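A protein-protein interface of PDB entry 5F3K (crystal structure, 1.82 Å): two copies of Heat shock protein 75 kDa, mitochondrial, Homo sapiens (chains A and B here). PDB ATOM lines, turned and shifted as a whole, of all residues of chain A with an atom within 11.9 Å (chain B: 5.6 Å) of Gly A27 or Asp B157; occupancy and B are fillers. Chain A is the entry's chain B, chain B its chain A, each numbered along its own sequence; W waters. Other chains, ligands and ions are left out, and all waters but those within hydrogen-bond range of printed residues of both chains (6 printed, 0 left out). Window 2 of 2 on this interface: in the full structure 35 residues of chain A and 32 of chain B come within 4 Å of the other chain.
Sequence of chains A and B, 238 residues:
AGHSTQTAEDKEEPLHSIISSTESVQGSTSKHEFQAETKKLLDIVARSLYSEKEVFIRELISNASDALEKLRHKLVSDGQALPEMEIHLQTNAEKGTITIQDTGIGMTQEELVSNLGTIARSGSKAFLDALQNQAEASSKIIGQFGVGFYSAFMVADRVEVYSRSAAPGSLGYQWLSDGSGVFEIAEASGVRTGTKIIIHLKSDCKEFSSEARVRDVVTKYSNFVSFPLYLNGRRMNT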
ATOM      1  N   GLN A  26     -15.493  23.930  29.439  1.00  0.00           N
ATOM      2  CA  GLN A  26     -16.850  23.520  28.963  1.00  0.00           C
ATOM      3  C   GLN A  26     -16.812  22.935  27.546  1.00  0.00           C
ATOM      4  O   GLN A  26     -17.394  21.878  27.301  1.00  0.00           O
ATOM      5  CB  GLN A  26     -17.834  24.690  29.043  1.00  0.00           C
ATOM      6  CG  GLN A  26     -19.049  24.545  28.145  1.00  0.00           C
ATOM      7  CD  GLN A  26     -20.332  24.271  28.921  1.00  0.00           C
ATOM      8  OE1 GLN A  26     -20.580  24.879  29.964  1.00  0.00           O
ATOM      9  NE2 GLN A  26     -21.211  23.456  28.339  1.00  0.00           N
ATOM     10  N   GLY A  27     -16.061  23.575  26.651  1.00  0.00           N
ATOM     11  CA  GLY A  27     -15.841  23.043  25.297  1.00  0.00           C
ATOM     12  C   GLY A  27     -14.542  22.266  25.162  1.00  0.00           C
ATOM     13  O   GLY A  27     -13.557  22.578  25.811  1.00  0.00           O
ATOM     14  N   SER A  28     -14.549  21.215  24.347  1.00  0.00           N
ATOM     15  CA  SER A  28     -13.316  20.485  24.052  1.00  0.00           C
ATOM     16  C   SER A  28     -12.798  20.845  22.650  1.00  0.00           C
ATOM     17  O   SER A  28     -13.572  21.293  21.801  1.00  0.00           O
ATOM     18  CB  SER A  28     -13.578  18.981  24.146  1.00  0.00           C
ATOM     19  OG  SER A  28     -14.738  18.639  23.404  1.00  0.00           O
ATOM     20  N   THR A  29     -11.522  20.565  22.379  1.00  0.00           N
ATOM     21  CA  THR A  29     -10.990  20.765  21.027  1.00  0.00           C
ATOM     22  C   THR A  29     -11.397  19.632  20.097  1.00  0.00           C
ATOM     23  O   THR A  29     -11.612  18.506  20.537  1.00  0.00           O
ATOM     24  CB  THR A  29      -9.441  20.930  20.992  1.00  0.00           C
ATOM     25  OG1 THR A  29      -8.792  19.712  21.390  1.00  0.00           O
ATOM     26  CG2 THR A  29      -9.003  22.078  21.887  1.00  0.00           C
ATOM     27  N   SER A  30     -11.568  19.956  18.822  1.00  0.00           N
ATOM     28  CA  SER A  30     -11.806  18.930  17.816  1.00  0.00           C
ATOM     29  C   SER A  30     -10.674  17.897  17.789  1.00  0.00           C
ATOM     30  O   SER A  30     -10.919  16.684  17.734  1.00  0.00           O
ATOM     31  CB  SER A  30     -11.984  19.578  16.444  1.00  0.00           C
ATOM     32  OG  SER A  30     -12.378  18.615  15.496  1.00  0.00           O
ATOM     33  N   LYS A  31      -9.442  18.369  17.955  1.00  0.00           N
ATOM     34  CA  LYS A  31      -8.287  17.468  17.954  1.00  0.00           C
ATOM     35  C   LYS A  31      -8.398  16.433  19.073  1.00  0.00           C
ATOM     36  O   LYS A  31      -8.209  15.240  18.838  1.00  0.00           O
ATOM     37  CB  LYS A  31      -6.982  18.254  18.074  1.00  0.00           C
ATOM     38  CG  LYS A  31      -5.734  17.405  17.862  1.00  0.00           C
ATOM     39  CD  LYS A  31      -4.485  18.277  17.811  1.00  0.00           C
ATOM     40  CE  LYS A  31      -3.350  17.582  17.081  1.00  0.00           C
ATOM     41  NZ  LYS A  31      -2.159  18.469  16.941  1.00  0.00           N
ATOM     42  N   HIS A  32      -8.760  16.879  20.277  1.00  0.00           N
ATOM     43  CA  HIS A  32      -8.893  15.957  21.402  1.00  0.00           C
ATOM     44  C   HIS A  32     -10.025  14.960  21.167  1.00  0.00           C
ATOM     45  O   HIS A  32      -9.930  13.789  21.550  1.00  0.00           O
ATOM     46  CB  HIS A  32      -9.120  16.719  22.708  1.00  0.00           C
ATOM     47  CG  HIS A  32      -7.864  17.263  23.314  1.00  0.00           C
ATOM     48  ND1 HIS A  32      -7.871  18.326  24.190  1.00  0.00           N
ATOM     49  CD2 HIS A  32      -6.563  17.007  23.045  1.00  0.00           C
ATOM     50  CE1 HIS A  32      -6.628  18.633  24.518  1.00  0.00           C
ATOM     51  NE2 HIS A  32      -5.813  17.874  23.810  1.00  0.00           N
ATOM     52  N   GLU A  33     -11.135  15.447  20.623  1.00  0.00           N
ATOM     53  CA  GLU A  33     -12.252  14.565  20.300  1.00  0.00           C
ATOM     54  C   GLU A  33     -11.878  13.502  19.256  1.00  0.00           C
ATOM     55  O   GLU A  33     -12.263  12.343  19.389  1.00  0.00           O
ATOM     56  CB  GLU A  33     -13.473  15.375  19.855  1.00  0.00           C
ATOM     57  CG  GLU A  33     -13.981  16.305  20.952  1.00  0.00           C
ATOM     58  CD  GLU A  33     -14.674  15.552  22.087  1.00  0.00           C
ATOM     59  OE1 GLU A  33     -14.795  14.312  21.989  1.00  0.00           O
ATOM     60  OE2 GLU A  33     -15.054  16.199  23.093  1.00  0.00           O
ATOM     61  N   PHE A  34     -11.170  13.889  18.196  1.00  0.00           N
ATOM     62  CA  PHE A  34     -10.776  12.901  17.187  1.00  0.00           C
ATOM     63  C   PHE A  34      -9.886  11.836  17.823  1.00  0.00           C
ATOM     64  O   PHE A  34      -9.992  10.644  17.516  1.00  0.00           O
ATOM     65  CB  PHE A  34     -10.052  13.566  16.004  1.00  0.00           C
ATOM     66  CG  PHE A  34     -10.980  14.028  14.917  1.00  0.00           C
ATOM     67  CD1 PHE A  34     -11.498  13.123  13.999  1.00  0.00           C
ATOM     68  CD2 PHE A  34     -11.422  15.341  14.893  1.00  0.00           C
ATOM     69  CE1 PHE A  34     -12.401  13.533  13.030  1.00  0.00           C
ATOM     70  CE2 PHE A  34     -12.403  15.741  14.002  1.00  0.00           C
ATOM     71  CZ  PHE A  34     -12.834  14.859  13.015  1.00  0.00           C
ATOM     72  N   VAL B 155     -16.899  18.958  15.112  1.00  0.00           N
ATOM     73  CA  VAL B 155     -16.368  20.311  14.941  1.00  0.00           C
ATOM     74  C   VAL B 155     -17.123  21.362  15.770  1.00  0.00           C
ATOM     75  O   VAL B 155     -16.833  22.561  15.687  1.00  0.00           O
ATOM     76  CB  VAL B 155     -16.316  20.743  13.458  1.00  0.00           C
ATOM     77  CG1 VAL B 155     -15.351  19.801  12.664  1.00  0.00           C
ATOM     78  CG2 VAL B 155     -17.712  20.768  12.845  1.00  0.00           C
ATOM     79  N   ALA B 156     -18.144  20.916  16.493  1.00  0.00           N
ATOM     80  CA  ALA B 156     -19.125  21.839  17.097  1.00  0.00           C
ATOM     81  C   ALA B 156     -18.975  21.871  18.620  1.00  0.00           C
ATOM     82  O   ALA B 156     -18.998  20.814  19.254  1.00  0.00           O
ATOM     83  CB  ALA B 156     -20.524  21.394  16.731  1.00  0.00           C
ATOM     84  N   ASP B 157     -19.053  23.070  19.213  1.00  0.00           N
ATOM     85  CA  ASP B 157     -19.434  23.210  20.627  1.00  0.00           C
ATOM     86  C   ASP B 157     -20.948  23.042  20.782  1.00  0.00           C
ATOM     87  O   ASP B 157     -21.431  22.662  21.849  1.00  0.00           O
ATOM     88  CB  ASP B 157     -19.082  24.617  21.146  1.00  0.00           C
ATOM     89  CG  ASP B 157     -17.594  24.843  21.321  1.00  0.00           C
ATOM     90  OD1 ASP B 157     -16.871  23.879  21.665  1.00  0.00           O
ATOM     91  OD2 ASP B 157     -17.225  26.039  21.425  1.00  0.00           O
ATOM     92  N   ARG B 158     -21.693  23.580  19.823  1.00  0.00           N
ATOM     93  CA  ARG B 158     -23.146  23.617  19.946  1.00  0.00           C
ATOM     94  C   ARG B 158     -23.751  23.354  18.581  1.00  0.00           C
ATOM     95  O   ARG B 158     -23.259  23.865  17.568  1.00  0.00           O
ATOM     96  CB  ARG B 158     -23.560  24.991  20.497  1.00  0.00           C
ATOM     97  CG  ARG B 158     -25.033  25.232  20.664  1.00  0.00           C
ATOM     98  CD  ARG B 158     -25.244  26.677  21.147  1.00  0.00           C
ATOM     99  NE  ARG B 158     -26.650  26.979  21.384  1.00  0.00           N
ATOM    100  CZ  ARG B 158     -27.232  26.860  22.573  1.00  0.00           C
ATOM    101  NH1 ARG B 158     -26.507  26.498  23.628  1.00  0.00           N
ATOM    102  NH2 ARG B 158     -28.527  27.104  22.706  1.00  0.00           N
ATOM    103  N   VAL B 159     -24.766  22.499  18.532  1.00  0.00           N
ATOM    104  CA  VAL B 159     -25.470  22.237  17.275  1.00  0.00           C
ATOM    105  C   VAL B 159     -26.959  22.499  17.432  1.00  0.00           C
ATOM    106  O   VAL B 159     -27.590  21.940  18.320  1.00  0.00           O
ATOM    107  CB  VAL B 159     -25.303  20.776  16.815  1.00  0.00           C
ATOM    108  CG1 VAL B 159     -26.020  20.578  15.499  1.00  0.00           C
ATOM    109  CG2 VAL B 159     -23.818  20.407  16.693  1.00  0.00           C
ATOM    110  N   SER B 177     -28.159  20.404  20.742  1.00  0.00           N
ATOM    111  CA  SER B 177     -27.073  19.859  21.569  1.00  0.00           C
ATOM    112  C   SER B 177     -26.158  20.992  21.987  1.00  0.00           C
ATOM    113  O   SER B 177     -25.560  21.657  21.133  1.00  0.00           O
ATOM    114  CB  SER B 177     -26.262  18.834  20.787  1.00  0.00           C
ATOM    115  OG  SER B 177     -25.144  18.387  21.558  1.00  0.00           O
ATOM    116  N   ASP B 178     -26.002  21.180  23.293  1.00  0.00           N
ATOM    117  CA  ASP B 178     -25.199  22.289  23.799  1.00  0.00           C
ATOM    118  C   ASP B 178     -23.881  21.778  24.389  1.00  0.00           C
ATOM    119  O   ASP B 178     -23.095  22.549  24.944  1.00  0.00           O
ATOM    120  CB  ASP B 178     -25.983  23.091  24.834  1.00  0.00           C
ATOM    121  CG  ASP B 178     -26.246  22.302  26.101  1.00  0.00           C
ATOM    122  OD1 ASP B 178     -26.742  22.896  27.082  1.00  0.00           O
ATOM    123  OD2 ASP B 178     -25.846  21.120  26.156  1.00  0.00           O
ATOM    124  N   GLY B 179     -23.604  20.497  24.174  1.00  0.00           N
ATOM    125  CA  GLY B 179     -22.321  19.909  24.557  1.00  0.00           C
ATOM    126  C   GLY B 179     -22.322  19.311  25.953  1.00  0.00           C
ATOM    127  O   GLY B 179     -21.303  18.784  26.416  1.00  0.00           O
ATOM    128  N   HIS B 200     -22.083  26.100  16.018  1.00  0.00           N
ATOM    129  CA  HIS B 200     -21.109  26.962  16.706  1.00  0.00           C
ATOM    130  C   HIS B 200     -19.797  26.196  16.825  1.00  0.00           C
ATOM    131  O   HIS B 200     -19.730  25.178  17.503  1.00  0.00           O
ATOM    132  CB  HIS B 200     -21.602  27.342  18.108  1.00  0.00           C
ATOM    133  CG  HIS B 200     -22.851  28.172  18.109  1.00  0.00           C
ATOM    134  ND1 HIS B 200     -24.070  27.685  17.692  1.00  0.00           N
ATOM    135  CD2 HIS B 200     -23.051  29.476  18.409  1.00  0.00           C
ATOM    136  CE1 HIS B 200     -24.969  28.654  17.736  1.00  0.00           C
ATOM    137  NE2 HIS B 200     -24.380  29.746  18.188  1.00  0.00           N
ATOM    138  N   LEU B 201     -18.772  26.668  16.128  1.00  0.00           N
ATOM    139  CA  LEU B 201     -17.574  25.865  15.894  1.00  0.00           C
ATOM    140  C   LEU B 201     -16.678  25.786  17.128  1.00  0.00           C
ATOM    141  O   LEU B 201     -16.617  26.737  17.921  1.00  0.00           O
ATOM    142  CB  LEU B 201     -16.798  26.441  14.703  1.00  0.00           C
ATOM    143  CG  LEU B 201     -17.546  26.280  13.376  1.00  0.00           C
ATOM    144  CD1 LEU B 201     -17.147  27.382  12.396  1.00  0.00           C
ATOM    145  CD2 LEU B 201     -17.270  24.888  12.773  1.00  0.00           C
ATOM    146  N   LYS B 202     -16.009  24.640  17.308  1.00  0.00           N
ATOM    147  CA  LYS B 202     -15.048  24.467  18.396  1.00  0.00           C
ATOM    148  C   LYS B 202     -13.889  25.458  18.273  1.00  0.00           C
ATOM    149  O   LYS B 202     -13.666  26.041  17.202  1.00  0.00           O
ATOM    150  CB  LYS B 202     -14.507  23.025  18.402  1.00  0.00           C
ATOM    151  CG  LYS B 202     -15.548  21.969  18.836  1.00  0.00           C
ATOM    152  CD  LYS B 202     -14.974  20.561  18.745  1.00  0.00           C
ATOM    153  CE  LYS B 202     -15.951  19.535  19.315  1.00  0.00           C
ATOM    154  NZ  LYS B 202     -16.191  19.755  20.774  1.00  0.00           N
ATOM    155  N   SER B 203     -13.043  25.478  19.297  1.00  0.00           N
ATOM    156  CA  SER B 203     -12.014  26.505  19.432  1.00  0.00           C
ATOM    157  C   SER B 203     -10.933  26.342  18.378  1.00  0.00           C
ATOM    158  O   SER B 203     -10.362  27.330  17.905  1.00  0.00           O
ATOM    159  CB  SER B 203     -11.386  26.431  20.826  1.00  0.00           C
ATOM    160  OG  SER B 203     -10.644  25.224  20.967  1.00  0.00           O
HETATM  161  O   HOH W   1     -17.024  21.539  22.456  1.00  0.00           O
HETATM  162  O   HOH W   2     -18.663  19.262  28.130  1.00  0.00           O
HETATM  163  O   HOH W   3     -17.473  17.470  21.841  1.00  0.00           O
HETATM  164  O   HOH W   4     -18.831  20.719  25.150  1.00  0.00           O
HETATM  165  O   HOH W   5     -16.599  26.251  24.568  1.00  0.00           O
HETATM  166  O   HOH W   6     -14.072  24.161  21.670  1.00  0.00           O
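The side-chain hydroxyl (OG) of Ser A28 is in hydrogen-bond range of the side-chain amino group (NZ) of Lys B202 (3.2 Å).
The backbone NH (N) of Asp B157 is in hydrogen-bond range of the backbone carbonyl oxygen (O) of His B200, at 2.8 Å. The side-chain hydroxyl of Ser A28 sits at hydrogen-bond distance from the side-chain carboxylate of Glu A33, at 2.5 Å. The side-chain hydroxyl (OG1) of Thr A29 sits at hydrogen-bond distance from the backbone NH (N) of His A32 (3.0 Å). The backbone carbonyl oxygen of Ala B156 lies close to the side-chain amino group of Lys B202 (3.4 Å). The backbone NH (N) of Lys B202 sits at hydrogen-bond distance from the backbone carbonyl oxygen (O) of Val B155, at 2.8 Å.
Asp B178 touches Gln A26. CA of Gly A27 touches OD1 of Asp B157, at 3.9 Å. Lys B202 touches Thr A29 (CD to C, 3.9 Å). Thr A29 touches Ser B203. Lys B202 touches Ser A30.
Of the printed residues of chain B, Gln A26 touches Asp B178. Gly A27 touches just one residue of chain B: Asp B157. Of the printed residues of chain B, Ser A28 touches Lys B202. Of the printed residues of chain B, Thr A29 touches Lys B202 (3.9 Å) and Ser B203 (3.7 Å). Printed residues of chain B within 4 Å of Ser A30: Lys B202. His A32 touches none of the printed residues of chain B. Val B155 touches none of the printed residues of chain A. Ala B156 touches none of the printed residues of chain A. Asp B157 touches just one residue of chain A: Gly A27 (3.9 Å). No residue of chain A comes within 4 Å of Val B159. No residue of chain A comes within 4 Å of Ser B177. Of the printed residues of chain A, Asp B178 touches Gln A26. Gly B179 touches none of the printed residues of chain A. Ser B203 touches just one residue of chain A: Thr A29 (3.7 Å). The nearest residue of chain A that does not touch Asp B157 is Ser A28 (4.2 Å).
Of the 9 printed residues of chain A, 5 touch a printed residue of chain B. Printed residues of chain A that touch a printed residue of chain B: Gln A26, Gly A27, Ser A28, Thr A29 and Ser A30. Printed residues of chain B that touch a printed residue of chain A: Asp B157, Asp B178, Lys B202 and Ser B203.
No position is printed for both chains.
Water W1 lies within hydrogen-bond range of the side-chain carboxylate of Asp B157, the side-chain amino group of Lys B202 and the backbone NH of Ser A28. Water W6 lies within hydrogen-bond range of the side-chain carboxylate (OD1) of Asp B157 (2.8 Å), the backbone NH (N) of Ser B203 (2.9 Å) and the backbone carbonyl oxygen (O) of Ser A28 (2.9 Å). Water W3 lies within hydrogen-bond range of NZ of Lys B202, OE2 of Glu A33 and OG of Ser A28. Water W4 bridges the backbone carbonyl oxygen of Gln A26 (2.8 Å) and the backbone carbonyl oxygen of Gly B179 (3.4 Å). Water W2 lies within hydrogen-bond range of O of Gln A26 (3.0 Å) and O of Gly B179 (3.2 Å). Water W5 lies within hydrogen-bond range of OD2 of Asp B157 (3.2 Å) and N of Gly A27 (3.4 Å).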
